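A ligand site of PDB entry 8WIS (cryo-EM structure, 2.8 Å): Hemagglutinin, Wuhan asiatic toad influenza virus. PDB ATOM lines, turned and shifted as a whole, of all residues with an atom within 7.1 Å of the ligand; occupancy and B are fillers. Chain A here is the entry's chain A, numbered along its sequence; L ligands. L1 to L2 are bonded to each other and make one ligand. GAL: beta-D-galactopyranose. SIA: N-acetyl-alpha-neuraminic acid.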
ATOM      1  N   GLY A 126     -18.559  10.659  -7.066  1.00  0.00           N
ATOM      2  CA  GLY A 126     -18.673  11.153  -8.414  1.00  0.00           C
ATOM      3  C   GLY A 126     -20.096  11.546  -8.752  1.00  0.00           C
ATOM      4  O   GLY A 126     -21.064  10.982  -8.222  1.00  0.00           O
ATOM      5  N   ALA A 127     -20.234  12.511  -9.645  1.00  0.00           N
ATOM      6  CA  ALA A 127     -21.522  13.055 -10.025  1.00  0.00           C
ATOM      7  C   ALA A 127     -21.725  12.922 -11.526  1.00  0.00           C
ATOM      8  O   ALA A 127     -20.814  13.209 -12.312  1.00  0.00           O
ATOM      9  CB  ALA A 127     -21.652  14.523  -9.619  1.00  0.00           C
ATOM     10  N   THR A 128     -22.918  12.474 -11.915  1.00  0.00           N
ATOM     11  CA  THR A 128     -23.278  12.376 -13.329  1.00  0.00           C
ATOM     12  C   THR A 128     -24.770  12.663 -13.460  1.00  0.00           C
ATOM     13  O   THR A 128     -25.550  12.391 -12.547  1.00  0.00           O
ATOM     14  CB  THR A 128     -22.939  10.999 -13.911  1.00  0.00           C
ATOM     15  OG1 THR A 128     -23.413  10.927 -15.264  1.00  0.00           O
ATOM     16  CG2 THR A 128     -23.579   9.900 -13.088  1.00  0.00           C
ATOM     17  N   SER A 129     -25.149  13.207 -14.619  1.00  0.00           N
ATOM     18  CA  SER A 129     -26.541  13.585 -14.842  1.00  0.00           C
ATOM     19  C   SER A 129     -27.403  12.414 -15.302  1.00  0.00           C
ATOM     20  O   SER A 129     -28.627  12.512 -15.259  1.00  0.00           O
ATOM     21  CB  SER A 129     -26.622  14.703 -15.876  1.00  0.00           C
ATOM     22  OG  SER A 129     -26.349  14.223 -17.177  1.00  0.00           O
ATOM     23  N   GLU A 130     -26.789  11.309 -15.736  1.00  0.00           N
ATOM     24  CA  GLU A 130     -27.561  10.158 -16.186  1.00  0.00           C
ATOM     25  C   GLU A 130     -28.161   9.374 -15.024  1.00  0.00           C
ATOM     26  O   GLU A 130     -29.083   8.574 -15.251  1.00  0.00           O
ATOM     27  CB  GLU A 130     -26.674   9.231 -17.028  1.00  0.00           C
ATOM     28  CG  GLU A 130     -25.886   9.959 -18.098  1.00  0.00           C
ATOM     29  CD  GLU A 130     -25.158   9.009 -19.028  1.00  0.00           C
ATOM     30  OE1 GLU A 130     -25.177   7.795 -18.760  1.00  0.00           O
ATOM     31  OE2 GLU A 130     -24.557   9.481 -20.014  1.00  0.00           O
ATOM     32  N   TRP A 139     -19.363   6.618  -6.269  1.00  0.00           N
ATOM     33  CA  TRP A 139     -18.481   6.576  -7.438  1.00  0.00           C
ATOM     34  C   TRP A 139     -17.142   7.205  -7.064  1.00  0.00           C
ATOM     35  O   TRP A 139     -17.073   8.397  -6.785  1.00  0.00           O
ATOM     36  CB  TRP A 139     -19.119   7.311  -8.620  1.00  0.00           C
ATOM     37  CG  TRP A 139     -18.508   6.984  -9.932  1.00  0.00           C
ATOM     38  CD1 TRP A 139     -17.625   5.978 -10.198  1.00  0.00           C
ATOM     39  CD2 TRP A 139     -18.733   7.656 -11.179  1.00  0.00           C
ATOM     40  NE1 TRP A 139     -17.278   5.983 -11.531  1.00  0.00           N
ATOM     41  CE2 TRP A 139     -17.950   7.001 -12.154  1.00  0.00           C
ATOM     42  CE3 TRP A 139     -19.522   8.734 -11.563  1.00  0.00           C
ATOM     43  CZ2 TRP A 139     -17.929   7.405 -13.478  1.00  0.00           C
ATOM     44  CZ3 TRP A 139     -19.506   9.132 -12.881  1.00  0.00           C
ATOM     45  CH2 TRP A 139     -18.717   8.466 -13.829  1.00  0.00           C
ATOM     46  N   VAL A 141     -13.926   8.674  -7.915  1.00  0.00           N
ATOM     47  CA  VAL A 141     -13.146   9.323  -8.964  1.00  0.00           C
ATOM     48  C   VAL A 141     -12.243  10.388  -8.346  1.00  0.00           C
ATOM     49  O   VAL A 141     -12.587  11.583  -8.357  1.00  0.00           O
ATOM     50  CB  VAL A 141     -14.057   9.903 -10.064  1.00  0.00           C
ATOM     51  CG1 VAL A 141     -14.603   8.782 -10.909  1.00  0.00           C
ATOM     52  CG2 VAL A 141     -15.208  10.661  -9.452  1.00  0.00           C
ATOM     53  N   LYS A 145      -5.854  10.524 -10.707  1.00  0.00           N
ATOM     54  CA  LYS A 145      -6.216   9.245 -11.284  1.00  0.00           C
ATOM     55  C   LYS A 145      -4.966   8.472 -11.689  1.00  0.00           C
ATOM     56  O   LYS A 145      -4.004   9.058 -12.180  1.00  0.00           O
ATOM     57  CB  LYS A 145      -7.115   9.466 -12.504  1.00  0.00           C
ATOM     58  CG  LYS A 145      -8.353  10.278 -12.185  1.00  0.00           C
ATOM     59  CD  LYS A 145      -9.161  10.589 -13.433  1.00  0.00           C
ATOM     60  CE  LYS A 145     -10.389  11.397 -13.092  1.00  0.00           C
ATOM     61  NZ  LYS A 145     -10.039  12.749 -12.597  1.00  0.00           N
ATOM     62  N   LEU A 166     -18.263   1.498 -13.065  1.00  0.00           N
ATOM     63  CA  LEU A 166     -19.251   2.330 -13.753  1.00  0.00           C
ATOM     64  C   LEU A 166     -18.501   3.062 -14.869  1.00  0.00           C
ATOM     65  O   LEU A 166     -17.840   4.061 -14.605  1.00  0.00           O
ATOM     66  CB  LEU A 166     -19.940   3.298 -12.802  1.00  0.00           C
ATOM     67  CG  LEU A 166     -20.847   4.337 -13.440  1.00  0.00           C
ATOM     68  CD1 LEU A 166     -21.973   3.651 -14.181  1.00  0.00           C
ATOM     69  CD2 LEU A 166     -21.400   5.278 -12.389  1.00  0.00           C
ATOM     70  N   LEU A 167     -18.611   2.565 -16.088  1.00  0.00           N
ATOM     71  CA  LEU A 167     -17.805   3.054 -17.199  1.00  0.00           C
ATOM     72  C   LEU A 167     -18.682   3.369 -18.393  1.00  0.00           C
ATOM     73  O   LEU A 167     -19.692   2.704 -18.640  1.00  0.00           O
ATOM     74  CB  LEU A 167     -16.741   2.031 -17.597  1.00  0.00           C
ATOM     75  CG  LEU A 167     -15.850   1.504 -16.467  1.00  0.00           C
ATOM     76  CD1 LEU A 167     -15.328   0.120 -16.799  1.00  0.00           C
ATOM     77  CD2 LEU A 167     -14.713   2.456 -16.197  1.00  0.00           C
ATOM     78  N   SER A 168     -18.295   4.391 -19.148  1.00  0.00           N
ATOM     79  CA  SER A 168     -19.051   4.848 -20.301  1.00  0.00           C
ATOM     80  C   SER A 168     -18.747   3.952 -21.508  1.00  0.00           C
ATOM     81  O   SER A 168     -18.118   2.896 -21.391  1.00  0.00           O
ATOM     82  CB  SER A 168     -18.751   6.306 -20.591  1.00  0.00           C
ATOM     83  OG  SER A 168     -17.404   6.481 -21.001  1.00  0.00           O
ATOM     84  N   ASP A 169     -19.191   4.377 -22.685  1.00  0.00           N
ATOM     85  CA  ASP A 169     -18.969   3.642 -23.927  1.00  0.00           C
ATOM     86  C   ASP A 169     -17.892   4.258 -24.800  1.00  0.00           C
ATOM     87  O   ASP A 169     -17.025   3.547 -25.310  1.00  0.00           O
ATOM     88  CB  ASP A 169     -20.283   3.545 -24.724  1.00  0.00           C
ATOM     89  CG  ASP A 169     -21.071   2.300 -24.378  1.00  0.00           C
ATOM     90  OD1 ASP A 169     -20.463   1.338 -23.865  1.00  0.00           O
ATOM     91  OD2 ASP A 169     -22.291   2.290 -24.620  1.00  0.00           O
ATOM     92  N   ALA A 172     -13.250   8.358 -25.235  1.00  0.00           N
ATOM     93  CA  ALA A 172     -12.903   9.612 -24.577  1.00  0.00           C
ATOM     94  C   ALA A 172     -13.395   9.637 -23.135  1.00  0.00           C
ATOM     95  O   ALA A 172     -12.661  10.003 -22.221  1.00  0.00           O
ATOM     96  CB  ALA A 172     -13.487  10.791 -25.359  1.00  0.00           C
ATOM     97  N   GLY A 173     -14.643   9.223 -22.910  1.00  0.00           N
ATOM     98  CA  GLY A 173     -15.175   9.201 -21.558  1.00  0.00           C
ATOM     99  C   GLY A 173     -14.452   8.200 -20.676  1.00  0.00           C
ATOM    100  O   GLY A 173     -14.166   8.485 -19.509  1.00  0.00           O
ATOM    101  N   TYR A 174     -14.155   7.014 -21.207  1.00  0.00           N
ATOM    102  CA  TYR A 174     -13.440   6.011 -20.441  1.00  0.00           C
ATOM    103  C   TYR A 174     -12.059   6.509 -20.029  1.00  0.00           C
ATOM    104  O   TYR A 174     -11.645   6.345 -18.866  1.00  0.00           O
ATOM    105  CB  TYR A 174     -13.331   4.726 -21.248  1.00  0.00           C
ATOM    106  CG  TYR A 174     -12.551   3.617 -20.590  1.00  0.00           C
ATOM    107  CD1 TYR A 174     -13.178   2.703 -19.748  1.00  0.00           C
ATOM    108  CD2 TYR A 174     -11.192   3.461 -20.820  1.00  0.00           C
ATOM    109  CE1 TYR A 174     -12.460   1.681 -19.144  1.00  0.00           C
ATOM    110  CE2 TYR A 174     -10.470   2.446 -20.221  1.00  0.00           C
ATOM    111  CZ  TYR A 174     -11.111   1.563 -19.390  1.00  0.00           C
ATOM    112  OH  TYR A 174     -10.406   0.543 -18.793  1.00  0.00           O
ATOM    113  N   ALA A 176     -11.107   9.686 -19.785  1.00  0.00           N
ATOM    114  CA  ALA A 176     -11.247  10.805 -18.866  1.00  0.00           C
ATOM    115  C   ALA A 176     -11.627  10.348 -17.464  1.00  0.00           C
ATOM    116  O   ALA A 176     -11.248  10.987 -16.486  1.00  0.00           O
ATOM    117  CB  ALA A 176     -12.291  11.787 -19.402  1.00  0.00           C
ATOM    118  N   VAL A 177     -12.368   9.249 -17.348  1.00  0.00           N
ATOM    119  CA  VAL A 177     -12.792   8.774 -16.038  1.00  0.00           C
ATOM    120  C   VAL A 177     -11.686   7.966 -15.366  1.00  0.00           C
ATOM    121  O   VAL A 177     -11.250   8.304 -14.257  1.00  0.00           O
ATOM    122  CB  VAL A 177     -14.096   7.957 -16.147  1.00  0.00           C
ATOM    123  CG1 VAL A 177     -14.343   7.185 -14.870  1.00  0.00           C
ATOM    124  CG2 VAL A 177     -15.256   8.867 -16.460  1.00  0.00           C
ATOM    125  N   THR A 222     -30.492   7.656 -24.466  1.00  0.00           N
ATOM    126  CA  THR A 222     -29.391   8.604 -24.602  1.00  0.00           C
ATOM    127  C   THR A 222     -28.473   8.560 -23.386  1.00  0.00           C
ATOM    128  O   THR A 222     -28.037   9.592 -22.882  1.00  0.00           O
ATOM    129  CB  THR A 222     -29.908  10.018 -24.834  1.00  0.00           C
ATOM    130  OG1 THR A 222     -30.590  10.477 -23.655  1.00  0.00           O
ATOM    131  CG2 THR A 222     -30.875  10.062 -26.004  1.00  0.00           C
ATOM    132  N   ARG A 224     -24.900   6.539 -21.998  1.00  0.00           N
ATOM    133  CA  ARG A 224     -23.768   5.742 -22.423  1.00  0.00           C
ATOM    134  C   ARG A 224     -23.049   5.050 -21.264  1.00  0.00           C
ATOM    135  O   ARG A 224     -22.003   4.442 -21.483  1.00  0.00           O
ATOM    136  CB  ARG A 224     -22.778   6.619 -23.200  1.00  0.00           C
ATOM    137  CG  ARG A 224     -23.392   7.368 -24.362  1.00  0.00           C
ATOM    138  CD  ARG A 224     -23.081   6.690 -25.674  1.00  0.00           C
ATOM    139  NE  ARG A 224     -23.939   5.524 -25.895  1.00  0.00           N
ATOM    140  CZ  ARG A 224     -25.162   5.595 -26.396  1.00  0.00           C
ATOM    141  NH1 ARG A 224     -25.708   6.745 -26.756  1.00  0.00           N
ATOM    142  NH2 ARG A 224     -25.859   4.473 -26.555  1.00  0.00           N
ATOM    143  N   ASN A 225     -23.596   5.120 -20.063  1.00  0.00           N
ATOM    144  CA  ASN A 225     -22.936   4.583 -18.875  1.00  0.00           C
ATOM    145  C   ASN A 225     -23.451   3.188 -18.584  1.00  0.00           C
ATOM    146  O   ASN A 225     -24.648   2.929 -18.644  1.00  0.00           O
ATOM    147  CB  ASN A 225     -23.165   5.495 -17.674  1.00  0.00           C
ATOM    148  CG  ASN A 225     -22.117   6.588 -17.558  1.00  0.00           C
ATOM    149  OD1 ASN A 225     -21.010   6.346 -17.074  1.00  0.00           O
ATOM    150  ND2 ASN A 225     -22.459   7.784 -18.009  1.00  0.00           N
ATOM    151  N   ILE A 226     -22.520   2.287 -18.258  1.00  0.00           N
ATOM    152  CA  ILE A 226     -22.839   0.915 -17.883  1.00  0.00           C
ATOM    153  C   ILE A 226     -22.223   0.641 -16.522  1.00  0.00           C
ATOM    154  O   ILE A 226     -21.036   0.942 -16.297  1.00  0.00           O
ATOM    155  CB  ILE A 226     -22.318  -0.103 -18.928  1.00  0.00           C
ATOM    156  CG1 ILE A 226     -22.991   0.095 -20.286  1.00  0.00           C
ATOM    157  CG2 ILE A 226     -22.541  -1.522 -18.439  1.00  0.00           C
ATOM    158  CD1 ILE A 226     -22.291   1.079 -21.196  1.00  0.00           C
HETATM  159  C1  GAL L   1     -22.469  14.371 -22.967  1.00  0.00           C
HETATM  160  C2  GAL L   1     -23.862  13.898 -22.526  1.00  0.00           C
HETATM  161  C3  GAL L   1     -24.309  14.649 -21.277  1.00  0.00           C
HETATM  162  C4  GAL L   1     -23.265  14.479 -20.159  1.00  0.00           C
HETATM  163  C5  GAL L   1     -21.862  14.838 -20.691  1.00  0.00           C
HETATM  164  C6  GAL L   1     -20.732  14.494 -19.727  1.00  0.00           C
HETATM  165  O2  GAL L   1     -24.833  14.124 -23.534  1.00  0.00           O
HETATM  166  O3  GAL L   1     -25.538  14.141 -20.793  1.00  0.00           O
HETATM  167  O4  GAL L   1     -23.267  13.140 -19.688  1.00  0.00           O
HETATM  168  O5  GAL L   1     -21.546  14.144 -21.912  1.00  0.00           O
HETATM  169  O6  GAL L   1     -20.815  15.303 -18.562  1.00  0.00           O
HETATM  170  C1  SIA L   2     -21.891  13.959 -16.823  1.00  0.00           C
HETATM  171  C2  SIA L   2     -20.527  14.504 -17.398  1.00  0.00           C
HETATM  172  C3  SIA L   2     -19.729  15.386 -16.431  1.00  0.00           C
HETATM  173  C4  SIA L   2     -19.231  14.645 -15.197  1.00  0.00           C
HETATM  174  C5  SIA L   2     -18.411  13.414 -15.608  1.00  0.00           C
HETATM  175  C6  SIA L   2     -19.165  12.563 -16.659  1.00  0.00           C
HETATM  176  C7  SIA L   2     -18.192  11.573 -17.361  1.00  0.00           C
HETATM  177  C8  SIA L   2     -18.927  10.749 -18.435  1.00  0.00           C
HETATM  178  C9  SIA L   2     -18.659   9.256 -18.258  1.00  0.00           C
HETATM  179  C10 SIA L   2     -16.914  12.433 -13.855  1.00  0.00           C
HETATM  180  C11 SIA L   2     -15.769  13.178 -14.535  1.00  0.00           C
HETATM  181  N5  SIA L   2     -18.137  12.594 -14.427  1.00  0.00           N
HETATM  182  O1A SIA L   2     -22.441  14.613 -15.902  1.00  0.00           O
HETATM  183  O1B SIA L   2     -22.278  12.897 -17.392  1.00  0.00           O
HETATM  184  O4  SIA L   2     -18.365  15.462 -14.395  1.00  0.00           O
HETATM  185  O6  SIA L   2     -19.673  13.345 -17.728  1.00  0.00           O
HETATM  186  O7  SIA L   2     -17.099  12.288 -17.906  1.00  0.00           O
HETATM  187  O8  SIA L   2     -20.323  11.037 -18.415  1.00  0.00           O
HETATM  188  O9  SIA L   2     -19.903   8.562 -18.240  1.00  0.00           O
HETATM  189  O10 SIA L   2     -16.708  11.737 -12.867  1.00  0.00           O
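O1A of SIA L2 sits at hydrogen-bond distance from N of Ser 129, at 3.3 Å. OG1 of Thr 128 lies within hydrogen-bond range of O1B of SIA L2 (3.1 Å). The side-chain amide nitrogen (ND2) of Asn 225 is in hydrogen-bond range of an oxygen (O9) of SIA L2. A nitrogen (N5) of SIA L2 is in hydrogen-bond range of the backbone carbonyl oxygen (O) of Ala 127 (3.5 Å).
The side-chain carboxylate (OE1) of Glu 130 lies within hydrogen-bond range of the backbone NH (N) of Arg 224, 3.5 Å away. N of Tyr 174 lies within hydrogen-bond range of OG of Ser 168 (3.3 Å). The backbone carbonyl oxygen (O) of Trp 139 sits at hydrogen-bond distance from the backbone NH (N) of Gly 126, at 2.7 Å. The side-chain amide nitrogen (ND2) of Asn 225 sits at hydrogen-bond distance from the side-chain carboxylate (OE1) of Glu 130, at 2.8 Å. The backbone NH of Glu 130 lies close to the side-chain hydroxyl of Thr 128 (3.4 Å).
Residues that only touch the ligand: Ser 168 (3.5 Å), Trp 139 (3.8 Å), Val 177 (3.9 Å), Val 141 (3.9 Å) and Glu 130 (3.9 Å). Hydrophobic or aromatic side chains within 4 Å of the ligand: Trp 139, Val 141 and Val 177. The nearest printed residue that does not touch the ligand is Gly 173 (4.7 Å).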
